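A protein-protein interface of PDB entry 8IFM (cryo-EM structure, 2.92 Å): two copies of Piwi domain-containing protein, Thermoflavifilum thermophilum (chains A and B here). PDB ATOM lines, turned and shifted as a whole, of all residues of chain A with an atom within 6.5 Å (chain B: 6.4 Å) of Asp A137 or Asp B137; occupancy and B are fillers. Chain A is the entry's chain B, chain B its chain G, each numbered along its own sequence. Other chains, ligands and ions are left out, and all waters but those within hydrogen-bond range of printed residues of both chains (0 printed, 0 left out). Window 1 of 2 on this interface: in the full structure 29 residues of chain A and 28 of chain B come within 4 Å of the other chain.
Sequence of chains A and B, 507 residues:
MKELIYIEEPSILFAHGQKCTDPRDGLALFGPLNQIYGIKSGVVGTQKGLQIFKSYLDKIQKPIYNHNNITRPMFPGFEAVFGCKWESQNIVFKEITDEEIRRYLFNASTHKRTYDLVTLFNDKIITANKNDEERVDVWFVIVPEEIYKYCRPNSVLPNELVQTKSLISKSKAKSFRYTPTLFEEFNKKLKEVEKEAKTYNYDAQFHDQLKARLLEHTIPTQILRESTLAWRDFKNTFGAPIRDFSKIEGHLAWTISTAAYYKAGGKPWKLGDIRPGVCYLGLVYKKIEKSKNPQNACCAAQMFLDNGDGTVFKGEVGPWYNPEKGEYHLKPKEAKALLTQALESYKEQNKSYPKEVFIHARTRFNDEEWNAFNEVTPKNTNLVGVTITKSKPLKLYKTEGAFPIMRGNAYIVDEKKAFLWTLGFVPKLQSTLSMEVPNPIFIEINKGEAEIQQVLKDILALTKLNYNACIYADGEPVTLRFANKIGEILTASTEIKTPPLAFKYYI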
ATOM      1  N   ILE A  36     -21.203  11.015   9.682  1.00  0.00           N
ATOM      2  CA  ILE A  36     -21.082  10.489   8.331  1.00  0.00           C
ATOM      3  C   ILE A  36     -21.599  11.564   7.392  1.00  0.00           C
ATOM      4  O   ILE A  36     -22.542  12.293   7.721  1.00  0.00           O
ATOM      5  CB  ILE A  36     -21.845   9.161   8.171  1.00  0.00           C
ATOM      6  CG1 ILE A  36     -23.357   9.389   8.166  1.00  0.00           C
ATOM      7  CG2 ILE A  36     -21.458   8.192   9.271  1.00  0.00           C
ATOM      8  CD1 ILE A  36     -24.162   8.131   7.954  1.00  0.00           C
ATOM      9  N   TYR A  37     -20.953  11.709   6.241  1.00  0.00           N
ATOM     10  CA  TYR A  37     -21.276  12.832   5.376  1.00  0.00           C
ATOM     11  C   TYR A  37     -22.587  12.635   4.631  1.00  0.00           C
ATOM     12  O   TYR A  37     -23.154  13.612   4.133  1.00  0.00           O
ATOM     13  CB  TYR A  37     -20.123  13.066   4.406  1.00  0.00           C
ATOM     14  CG  TYR A  37     -18.799  13.182   5.122  1.00  0.00           C
ATOM     15  CD1 TYR A  37     -18.474  14.324   5.838  1.00  0.00           C
ATOM     16  CD2 TYR A  37     -17.886  12.138   5.105  1.00  0.00           C
ATOM     17  CE1 TYR A  37     -17.270  14.430   6.501  1.00  0.00           C
ATOM     18  CE2 TYR A  37     -16.680  12.235   5.764  1.00  0.00           C
ATOM     19  CZ  TYR A  37     -16.376  13.382   6.461  1.00  0.00           C
ATOM     20  OH  TYR A  37     -15.175  13.482   7.120  1.00  0.00           O
ATOM     21  N   GLY A  38     -23.087  11.409   4.568  1.00  0.00           N
ATOM     22  CA  GLY A  38     -24.350  11.150   3.912  1.00  0.00           C
ATOM     23  C   GLY A  38     -24.537   9.665   3.701  1.00  0.00           C
ATOM     24  O   GLY A  38     -23.677   8.848   4.042  1.00  0.00           O
ATOM     25  N   ILE A  39     -25.691   9.329   3.133  1.00  0.00           N
ATOM     26  CA  ILE A  39     -26.034   7.953   2.801  1.00  0.00           C
ATOM     27  C   ILE A  39     -26.263   7.883   1.299  1.00  0.00           C
ATOM     28  O   ILE A  39     -27.211   8.485   0.778  1.00  0.00           O
ATOM     29  CB  ILE A  39     -27.269   7.461   3.567  1.00  0.00           C
ATOM     30  CG1 ILE A  39     -27.041   7.562   5.075  1.00  0.00           C
ATOM     31  CG2 ILE A  39     -27.607   6.034   3.174  1.00  0.00           C
ATOM     32  CD1 ILE A  39     -28.266   7.233   5.887  1.00  0.00           C
ATOM     33  N   LYS A  40     -25.399   7.148   0.602  1.00  0.00           N
ATOM     34  CA  LYS A  40     -25.585   6.868  -0.820  1.00  0.00           C
ATOM     35  C   LYS A  40     -26.436   5.611  -0.917  1.00  0.00           C
ATOM     36  O   LYS A  40     -25.929   4.491  -0.989  1.00  0.00           O
ATOM     37  CB  LYS A  40     -24.244   6.717  -1.525  1.00  0.00           C
ATOM     38  CG  LYS A  40     -23.460   8.016  -1.628  1.00  0.00           C
ATOM     39  CD  LYS A  40     -22.497   8.006  -2.806  1.00  0.00           C
ATOM     40  CE  LYS A  40     -23.193   7.661  -4.113  1.00  0.00           C
ATOM     41  NZ  LYS A  40     -24.492   8.366  -4.276  1.00  0.00           N
ATOM     42  N   SER A  41     -27.751   5.802  -0.908  1.00  0.00           N
ATOM     43  CA  SER A  41     -28.671   4.679  -0.844  1.00  0.00           C
ATOM     44  C   SER A  41     -28.661   3.879  -2.140  1.00  0.00           C
ATOM     45  O   SER A  41     -28.670   4.439  -3.240  1.00  0.00           O
ATOM     46  CB  SER A  41     -30.088   5.171  -0.551  1.00  0.00           C
ATOM     47  OG  SER A  41     -30.411   6.293  -1.354  1.00  0.00           O
ATOM     48  N   GLY A  42     -28.638   2.561  -1.999  1.00  0.00           N
ATOM     49  CA  GLY A  42     -28.839   1.645  -3.110  1.00  0.00           C
ATOM     50  C   GLY A  42     -30.184   0.960  -2.944  1.00  0.00           C
ATOM     51  O   GLY A  42     -30.537   0.535  -1.842  1.00  0.00           O
ATOM     52  N   ARG A 135     -20.524   4.027  -5.689  1.00  0.00           N
ATOM     53  CA  ARG A 135     -20.394   3.495  -4.342  1.00  0.00           C
ATOM     54  C   ARG A 135     -21.714   3.619  -3.594  1.00  0.00           C
ATOM     55  O   ARG A 135     -22.407   4.634  -3.696  1.00  0.00           O
ATOM     56  CB  ARG A 135     -19.289   4.229  -3.586  1.00  0.00           C
ATOM     57  CG  ARG A 135     -19.138   3.824  -2.136  1.00  0.00           C
ATOM     58  CD  ARG A 135     -18.634   4.986  -1.304  1.00  0.00           C
ATOM     59  NE  ARG A 135     -19.715   5.860  -0.864  1.00  0.00           N
ATOM     60  CZ  ARG A 135     -19.552   7.124  -0.493  1.00  0.00           C
ATOM     61  NH1 ARG A 135     -18.363   7.702  -0.517  1.00  0.00           N
ATOM     62  NH2 ARG A 135     -20.606   7.821  -0.086  1.00  0.00           N
ATOM     63  N   VAL A 136     -22.059   2.580  -2.841  1.00  0.00           N
ATOM     64  CA  VAL A 136     -23.309   2.527  -2.094  1.00  0.00           C
ATOM     65  C   VAL A 136     -22.989   2.284  -0.627  1.00  0.00           C
ATOM     66  O   VAL A 136     -22.218   1.376  -0.296  1.00  0.00           O
ATOM     67  CB  VAL A 136     -24.249   1.439  -2.639  1.00  0.00           C
ATOM     68  CG1 VAL A 136     -25.437   1.251  -1.715  1.00  0.00           C
ATOM     69  CG2 VAL A 136     -24.712   1.807  -4.031  1.00  0.00           C
ATOM     70  N   ASP A 137     -23.582   3.099   0.247  1.00  0.00           N
ATOM     71  CA  ASP A 137     -23.345   2.969   1.679  1.00  0.00           C
ATOM     72  C   ASP A 137     -24.153   1.823   2.276  1.00  0.00           C
ATOM     73  O   ASP A 137     -23.634   1.055   3.093  1.00  0.00           O
ATOM     74  CB  ASP A 137     -23.687   4.283   2.377  1.00  0.00           C
ATOM     75  CG  ASP A 137     -22.532   5.259   2.374  1.00  0.00           C
ATOM     76  OD1 ASP A 137     -21.435   4.880   1.915  1.00  0.00           O
ATOM     77  OD2 ASP A 137     -22.723   6.409   2.822  1.00  0.00           O
ATOM     78  N   VAL A 138     -25.415   1.698   1.880  1.00  0.00           N
ATOM     79  CA  VAL A 138     -26.297   0.641   2.367  1.00  0.00           C
ATOM     80  C   VAL A 138     -27.360   0.375   1.309  1.00  0.00           C
ATOM     81  O   VAL A 138     -27.934   1.309   0.742  1.00  0.00           O
ATOM     82  CB  VAL A 138     -26.927   1.002   3.729  1.00  0.00           C
ATOM     83  CG1 VAL A 138     -27.563   2.370   3.678  1.00  0.00           C
ATOM     84  CG2 VAL A 138     -27.964  -0.036   4.120  1.00  0.00           C
ATOM     85  N   TRP A 139     -27.608  -0.903   1.034  1.00  0.00           N
ATOM     86  CA  TRP A 139     -28.514  -1.311  -0.030  1.00  0.00           C
ATOM     87  C   TRP A 139     -29.910  -1.522   0.543  1.00  0.00           C
ATOM     88  O   TRP A 139     -30.110  -2.397   1.389  1.00  0.00           O
ATOM     89  CB  TRP A 139     -28.011  -2.590  -0.696  1.00  0.00           C
ATOM     90  CG  TRP A 139     -26.894  -2.353  -1.652  1.00  0.00           C
ATOM     91  CD1 TRP A 139     -25.559  -2.451  -1.394  1.00  0.00           C
ATOM     92  CD2 TRP A 139     -27.011  -1.959  -3.021  1.00  0.00           C
ATOM     93  NE1 TRP A 139     -24.837  -2.153  -2.523  1.00  0.00           N
ATOM     94  CE2 TRP A 139     -25.706  -1.845  -3.534  1.00  0.00           C
ATOM     95  CE3 TRP A 139     -28.092  -1.695  -3.862  1.00  0.00           C
ATOM     96  CZ2 TRP A 139     -25.456  -1.480  -4.852  1.00  0.00           C
ATOM     97  CZ3 TRP A 139     -27.843  -1.334  -5.168  1.00  0.00           C
ATOM     98  CH2 TRP A 139     -26.537  -1.225  -5.649  1.00  0.00           C
ATOM     99  N   ILE A 219     -21.476  -6.435   2.923  1.00  0.00           N
ATOM    100  CA  ILE A 219     -22.320  -5.416   2.307  1.00  0.00           C
ATOM    101  C   ILE A 219     -23.463  -5.093   3.261  1.00  0.00           C
ATOM    102  O   ILE A 219     -24.377  -5.914   3.428  1.00  0.00           O
ATOM    103  CB  ILE A 219     -22.854  -5.879   0.941  1.00  0.00           C
ATOM    104  CG1 ILE A 219     -21.714  -6.002  -0.070  1.00  0.00           C
ATOM    105  CG2 ILE A 219     -23.923  -4.926   0.431  1.00  0.00           C
ATOM    106  CD1 ILE A 219     -22.109  -6.688  -1.355  1.00  0.00           C
ATOM    107  N   PRO A 220     -23.449  -3.937   3.920  1.00  0.00           N
ATOM    108  CA  PRO A 220     -24.582  -3.570   4.779  1.00  0.00           C
ATOM    109  C   PRO A 220     -25.842  -3.376   3.951  1.00  0.00           C
ATOM    110  O   PRO A 220     -25.859  -2.612   2.984  1.00  0.00           O
ATOM    111  CB  PRO A 220     -24.122  -2.263   5.436  1.00  0.00           C
ATOM    112  CG  PRO A 220     -23.009  -1.766   4.570  1.00  0.00           C
ATOM    113  CD  PRO A 220     -22.333  -2.986   4.049  1.00  0.00           C
ATOM    114  N   THR A 221     -26.903  -4.080   4.336  1.00  0.00           N
ATOM    115  CA  THR A 221     -28.157  -4.041   3.603  1.00  0.00           C
ATOM    116  C   THR A 221     -29.316  -3.914   4.581  1.00  0.00           C
ATOM    117  O   THR A 221     -29.254  -4.404   5.711  1.00  0.00           O
ATOM    118  CB  THR A 221     -28.345  -5.290   2.729  1.00  0.00           C
ATOM    119  OG1 THR A 221     -29.700  -5.357   2.270  1.00  0.00           O
ATOM    120  CG2 THR A 221     -28.016  -6.547   3.513  1.00  0.00           C
ATOM    121  N   LYS A 263     -26.538   1.500   9.385  1.00  0.00           N
ATOM    122  CA  LYS A 263     -25.982   0.674   8.322  1.00  0.00           C
ATOM    123  C   LYS A 263     -25.083   1.456   7.377  1.00  0.00           C
ATOM    124  O   LYS A 263     -24.379   0.841   6.568  1.00  0.00           O
ATOM    125  CB  LYS A 263     -27.114   0.000   7.548  1.00  0.00           C
ATOM    126  CG  LYS A 263     -27.929  -0.953   8.399  1.00  0.00           C
ATOM    127  CD  LYS A 263     -29.288  -1.227   7.795  1.00  0.00           C
ATOM    128  CE  LYS A 263     -29.852  -2.537   8.303  1.00  0.00           C
ATOM    129  NZ  LYS A 263     -29.478  -2.751   9.724  1.00  0.00           N
ATOM    130  N   ALA A 264     -25.085   2.782   7.461  1.00  0.00           N
ATOM    131  CA  ALA A 264     -24.198   3.622   6.674  1.00  0.00           C
ATOM    132  C   ALA A 264     -22.900   3.938   7.401  1.00  0.00           C
ATOM    133  O   ALA A 264     -22.112   4.752   6.910  1.00  0.00           O
ATOM    134  CB  ALA A 264     -24.908   4.919   6.285  1.00  0.00           C
ATOM    135  N   GLY A 265     -22.663   3.324   8.554  1.00  0.00           N
ATOM    136  CA  GLY A 265     -21.448   3.544   9.305  1.00  0.00           C
ATOM    137  C   GLY A 265     -21.535   4.571  10.409  1.00  0.00           C
ATOM    138  O   GLY A 265     -20.491   4.988  10.922  1.00  0.00           O
ATOM    139  N   TYR B  37     -21.193  12.383  -0.919  1.00  0.00           N
ATOM    140  CA  TYR B  37     -21.298  13.337   0.178  1.00  0.00           C
ATOM    141  C   TYR B  37     -19.979  13.531   0.912  1.00  0.00           C
ATOM    142  O   TYR B  37     -19.735  14.612   1.458  1.00  0.00           O
ATOM    143  CB  TYR B  37     -22.393  12.896   1.143  1.00  0.00           C
ATOM    144  CG  TYR B  37     -23.731  12.724   0.468  1.00  0.00           C
ATOM    145  CD1 TYR B  37     -24.529  13.822   0.188  1.00  0.00           C
ATOM    146  CD2 TYR B  37     -24.195  11.468   0.108  1.00  0.00           C
ATOM    147  CE1 TYR B  37     -25.750  13.677  -0.430  1.00  0.00           C
ATOM    148  CE2 TYR B  37     -25.417  11.313  -0.510  1.00  0.00           C
ATOM    149  CZ  TYR B  37     -26.191  12.421  -0.776  1.00  0.00           C
ATOM    150  OH  TYR B  37     -27.411  12.276  -1.392  1.00  0.00           O
ATOM    151  N   GLY B  38     -19.127  12.518   0.939  1.00  0.00           N
ATOM    152  CA  GLY B  38     -17.847  12.648   1.608  1.00  0.00           C
ATOM    153  C   GLY B  38     -17.096  11.340   1.543  1.00  0.00           C
ATOM    154  O   GLY B  38     -17.629  10.307   1.128  1.00  0.00           O
ATOM    155  N   ILE B  39     -15.838  11.400   1.963  1.00  0.00           N
ATOM    156  CA  ILE B  39     -14.961  10.238   1.987  1.00  0.00           C
ATOM    157  C   ILE B  39     -14.724   9.866   3.443  1.00  0.00           C
ATOM    158  O   ILE B  39     -14.118  10.632   4.202  1.00  0.00           O
ATOM    159  CB  ILE B  39     -13.642  10.502   1.252  1.00  0.00           C
ATOM    160  CG1 ILE B  39     -13.877  10.502  -0.257  1.00  0.00           C
ATOM    161  CG2 ILE B  39     -12.607   9.453   1.614  1.00  0.00           C
ATOM    162  CD1 ILE B  39     -13.237  11.655  -0.974  1.00  0.00           C
ATOM    163  N   LYS B  40     -15.213   8.689   3.834  1.00  0.00           N
ATOM    164  CA  LYS B  40     -14.957   8.128   5.159  1.00  0.00           C
ATOM    165  C   LYS B  40     -13.589   7.457   5.104  1.00  0.00           C
ATOM    166  O   LYS B  40     -13.456   6.239   4.975  1.00  0.00           O
ATOM    167  CB  LYS B  40     -16.059   7.150   5.550  1.00  0.00           C
ATOM    168  CG  LYS B  40     -17.378   7.794   5.977  1.00  0.00           C
ATOM    169  CD  LYS B  40     -17.287   8.546   7.294  1.00  0.00           C
ATOM    170  CE  LYS B  40     -16.420   7.817   8.310  1.00  0.00           C
ATOM    171  NZ  LYS B  40     -16.906   6.438   8.580  1.00  0.00           N
ATOM    172  N   SER B  41     -12.550   8.283   5.190  1.00  0.00           N
ATOM    173  CA  SER B  41     -11.193   7.802   4.975  1.00  0.00           C
ATOM    174  C   SER B  41     -10.793   6.787   6.037  1.00  0.00           C
ATOM    175  O   SER B  41     -10.973   7.016   7.236  1.00  0.00           O
ATOM    176  CB  SER B  41     -10.216   8.976   4.976  1.00  0.00           C
ATOM    177  OG  SER B  41     -10.595   9.952   5.930  1.00  0.00           O
ATOM    178  N   GLY B  42     -10.254   5.659   5.586  1.00  0.00           N
ATOM    179  CA  GLY B  42      -9.668   4.679   6.475  1.00  0.00           C
ATOM    180  C   GLY B  42      -8.192   4.527   6.184  1.00  0.00           C
ATOM    181  O   GLY B  42      -7.794   4.467   5.018  1.00  0.00           O
ATOM    182  N   ARG B 135     -17.858   2.911   8.885  1.00  0.00           N
ATOM    183  CA  ARG B 135     -17.736   2.641   7.460  1.00  0.00           C
ATOM    184  C   ARG B 135     -16.537   3.380   6.880  1.00  0.00           C
ATOM    185  O   ARG B 135     -16.224   4.502   7.286  1.00  0.00           O
ATOM    186  CB  ARG B 135     -19.015   3.052   6.727  1.00  0.00           C
ATOM    187  CG  ARG B 135     -18.801   3.554   5.307  1.00  0.00           C
ATOM    188  CD  ARG B 135     -20.122   3.755   4.587  1.00  0.00           C
ATOM    189  NE  ARG B 135     -20.796   4.982   4.996  1.00  0.00           N
ATOM    190  CZ  ARG B 135     -20.384   6.203   4.679  1.00  0.00           C
ATOM    191  NH1 ARG B 135     -19.336   6.398   3.897  1.00  0.00           N
ATOM    192  NH2 ARG B 135     -21.055   7.254   5.142  1.00  0.00           N
ATOM    193  N   VAL B 136     -15.860   2.738   5.932  1.00  0.00           N
ATOM    194  CA  VAL B 136     -14.752   3.336   5.203  1.00  0.00           C
ATOM    195  C   VAL B 136     -15.070   3.268   3.717  1.00  0.00           C
ATOM    196  O   VAL B 136     -15.415   2.199   3.202  1.00  0.00           O
ATOM    197  CB  VAL B 136     -13.421   2.629   5.510  1.00  0.00           C
ATOM    198  CG1 VAL B 136     -12.330   3.143   4.592  1.00  0.00           C
ATOM    199  CG2 VAL B 136     -13.040   2.831   6.965  1.00  0.00           C
ATOM    200  N   ASP B 137     -14.961   4.407   3.033  1.00  0.00           N
ATOM    201  CA  ASP B 137     -15.212   4.443   1.598  1.00  0.00           C
ATOM    202  C   ASP B 137     -13.998   4.026   0.783  1.00  0.00           C
ATOM    203  O   ASP B 137     -14.155   3.449  -0.298  1.00  0.00           O
ATOM    204  CB  ASP B 137     -15.652   5.842   1.161  1.00  0.00           C
ATOM    205  CG  ASP B 137     -16.912   6.302   1.860  1.00  0.00           C
ATOM    206  OD1 ASP B 137     -17.972   5.681   1.649  1.00  0.00           O
ATOM    207  OD2 ASP B 137     -16.852   7.308   2.593  1.00  0.00           O
ATOM    208  N   VAL B 138     -12.795   4.311   1.274  1.00  0.00           N
ATOM    209  CA  VAL B 138     -11.564   3.947   0.583  1.00  0.00           C
ATOM    210  C   VAL B 138     -10.444   3.901   1.614  1.00  0.00           C
ATOM    211  O   VAL B 138     -10.332   4.783   2.468  1.00  0.00           O
ATOM    212  CB  VAL B 138     -11.262   4.925  -0.578  1.00  0.00           C
ATOM    213  CG1 VAL B 138     -11.305   6.358  -0.096  1.00  0.00           C
ATOM    214  CG2 VAL B 138      -9.908   4.617  -1.196  1.00  0.00           C
ATOM    215  N   TRP B 139      -9.623   2.857   1.535  1.00  0.00           N
ATOM    216  CA  TRP B 139      -8.592   2.592   2.531  1.00  0.00           C
ATOM    217  C   TRP B 139      -7.251   3.093   2.014  1.00  0.00           C
ATOM    218  O   TRP B 139      -6.773   2.631   0.975  1.00  0.00           O
ATOM    219  CB  TRP B 139      -8.515   1.099   2.853  1.00  0.00           C
ATOM    220  CG  TRP B 139      -9.506   0.675   3.877  1.00  0.00           C
ATOM    221  CD1 TRP B 139     -10.766   0.207   3.654  1.00  0.00           C
ATOM    222  CD2 TRP B 139      -9.336   0.707   5.296  1.00  0.00           C
ATOM    223  NE1 TRP B 139     -11.387  -0.068   4.847  1.00  0.00           N
ATOM    224  CE2 TRP B 139     -10.529   0.233   5.870  1.00  0.00           C
ATOM    225  CE3 TRP B 139      -8.287   1.088   6.137  1.00  0.00           C
ATOM    226  CZ2 TRP B 139     -10.703   0.130   7.244  1.00  0.00           C
ATOM    227  CZ3 TRP B 139      -8.462   0.984   7.500  1.00  0.00           C
ATOM    228  CH2 TRP B 139      -9.659   0.510   8.041  1.00  0.00           C
ATOM    229  N   ILE B 219     -12.819  -4.083  -1.736  1.00  0.00           N
ATOM    230  CA  ILE B 219     -12.503  -2.935  -0.894  1.00  0.00           C
ATOM    231  C   ILE B 219     -11.652  -1.968  -1.708  1.00  0.00           C
ATOM    232  O   ILE B 219     -10.471  -2.249  -1.961  1.00  0.00           O
ATOM    233  CB  ILE B 219     -11.775  -3.365   0.389  1.00  0.00           C
ATOM    234  CG1 ILE B 219     -12.700  -4.193   1.281  1.00  0.00           C
ATOM    235  CG2 ILE B 219     -11.268  -2.152   1.147  1.00  0.00           C
ATOM    236  CD1 ILE B 219     -11.984  -4.885   2.414  1.00  0.00           C
ATOM    237  N   PRO B 220     -12.201  -0.839  -2.153  1.00  0.00           N
ATOM    238  CA  PRO B 220     -11.385   0.138  -2.888  1.00  0.00           C
ATOM    239  C   PRO B 220     -10.284   0.696  -2.000  1.00  0.00           C
ATOM    240  O   PRO B 220     -10.546   1.273  -0.944  1.00  0.00           O
ATOM    241  CB  PRO B 220     -12.407   1.210  -3.283  1.00  0.00           C
ATOM    242  CG  PRO B 220     -13.475   1.070  -2.238  1.00  0.00           C
ATOM    243  CD  PRO B 220     -13.607  -0.412  -2.098  1.00  0.00           C
ATOM    244  N   THR B 221      -9.043   0.509  -2.434  1.00  0.00           N
ATOM    245  CA  THR B 221      -7.880   0.901  -1.656  1.00  0.00           C
ATOM    246  C   THR B 221      -6.945   1.746  -2.505  1.00  0.00           C
ATOM    247  O   THR B 221      -6.843   1.563  -3.720  1.00  0.00           O
ATOM    248  CB  THR B 221      -7.125  -0.322  -1.115  1.00  0.00           C
ATOM    249  OG1 THR B 221      -5.844   0.084  -0.617  1.00  0.00           O
ATOM    250  CG2 THR B 221      -6.936  -1.360  -2.210  1.00  0.00           C
ATOM    251  N   LYS B 263     -11.975   6.383  -6.268  1.00  0.00           N
ATOM    252  CA  LYS B 263     -12.086   5.141  -5.514  1.00  0.00           C
ATOM    253  C   LYS B 263     -13.235   5.166  -4.517  1.00  0.00           C
ATOM    254  O   LYS B 263     -13.706   4.100  -4.109  1.00  0.00           O
ATOM    255  CB  LYS B 263     -10.771   4.842  -4.797  1.00  0.00           C
ATOM    256  CG  LYS B 263      -9.608   4.598  -5.741  1.00  0.00           C
ATOM    257  CD  LYS B 263      -8.284   4.883  -5.068  1.00  0.00           C
ATOM    258  CE  LYS B 263      -7.164   4.102  -5.722  1.00  0.00           C
ATOM    259  NZ  LYS B 263      -7.407   3.933  -7.177  1.00  0.00           N
ATOM    260  N   ALA B 264     -13.700   6.349  -4.117  1.00  0.00           N
ATOM    261  CA  ALA B 264     -14.837   6.475  -3.219  1.00  0.00           C
ATOM    262  C   ALA B 264     -16.164   6.560  -3.962  1.00  0.00           C
ATOM    263  O   ALA B 264     -17.154   7.037  -3.396  1.00  0.00           O
ATOM    264  CB  ALA B 264     -14.664   7.695  -2.315  1.00  0.00           C
ATOM    265  N   GLY B 265     -16.207   6.116  -5.215  1.00  0.00           N
ATOM    266  CA  GLY B 265     -17.448   6.095  -5.958  1.00  0.00           C
ATOM    267  C   GLY B 265     -17.816   7.386  -6.645  1.00  0.00           C
ATOM    268  O   GLY B 265     -18.981   7.566  -7.013  1.00  0.00           O
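NH1 of Arg A135 lies within hydrogen-bond range of O of Gly B38 (3.2 Å). NH1 of Arg A135 is in salt-bridge range of OD1 of Asp B137 (3.0 Å). O of Gly A38 lies within hydrogen-bond range of NH2 of Arg B135, at 3.3 Å. O of Ala A264 lies close to NH2 of Arg B135 (3.2 Å). NH1 of Arg A135 is in hydrogen-bond range of O of Ala B264 (3.2 Å). NH2 of Arg B135 lies within salt-bridge range of OD2 of Asp A137 (3.0 Å).
The backbone NH (N) of Asp A137 is in hydrogen-bond range of the backbone carbonyl oxygen (O) of Lys A40. O of Arg B135 is in hydrogen-bond range of NZ of Lys B40, at 2.4 Å. NE of Arg A135 lies within salt-bridge range of OD1 of Asp A137 (3.4 Å). The backbone NH (N) of Lys B40 is in hydrogen-bond range of the side-chain carboxylate (OD2) of Asp B137 (2.5 Å). The guanidinium group (NH1) of Arg B135 is in salt-bridge range of the side-chain carboxylate (OD1) of Asp B137, at 2.7 Å.
Among the printed residues, pairs that only touch across the chains: Tyr A37 with Tyr B37 (3.2 Å), Tyr A37 with Ile B39 (3.4 Å), Tyr A37 with Gly B38 (3.5 Å), Arg A135 with Gly B265 (3.5 Å), Asp A137 with Asp B137 (3.6 Å), Gly A265 with Arg B135 (3.6 Å), Ile A39 with Tyr B37 (3.6 Å), Ile A36 with Arg B135 (3.7 Å), Gly A38 with Tyr B37 (3.8 Å) and Lys A40 with Tyr B37 (3.9 Å).
Printed residues of chain B within 4 Å of Ile A36: Arg B135 (3.7 Å). Of the printed residues of chain B, Tyr A37 touches Tyr B37 (3.2 Å), Gly B38 (3.5 Å) and Ile B39 (3.4 Å). Of the printed residues of chain B, Arg A135 touches Gly B38 (3.2 Å), Asp B137 (3.0 Å), Ala B264 (3.2 Å) and Gly B265 (3.5 Å). Pro A220 touches none of the printed residues of chain B. Printed residues of chain A within 4 Å of Ile B39: Tyr A37 (3.4 Å). Pro B220 touches none of the printed residues of chain A. Printed residues of chain A within 4 Å of Gly B265: Arg A135 (3.5 Å). The nearest residue of chain B that does not touch Asp A137 is Tyr B37 (5.9 Å). The nearest residue of chain A that does not touch Asp B137 is Tyr A37 (5.5 Å).
Hydrophobic or aromatic side chains of chain A that line the printed part of chain B: Ile A36 and Tyr A37. Of the 17 printed residues of chain B, 7 touch a printed residue of chain A. Among the printed residues, Asp or Glu carboxylates within 4 Å of a Lys or Arg side-chain nitrogen of the other chain: Arg A135 with Asp B137 (3.0 Å) and Asp A137 with Arg B135 (3.0 Å).
Tyr B37 touches its own counterpart, Tyr A37. Tyr A37 touches Gly B38, and with the chains exchanged Gly A38 touches Tyr B37. Arg A135 touches Gly B265, and with the chains exchanged Gly A265 touches Arg B135. Asp A137 touches its own counterpart, Asp B137. 17 positions are printed for both chains. Of the 16 pairs that touch across the chains among the printed residues, 14 have their exchanged pair printed and touching as well.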
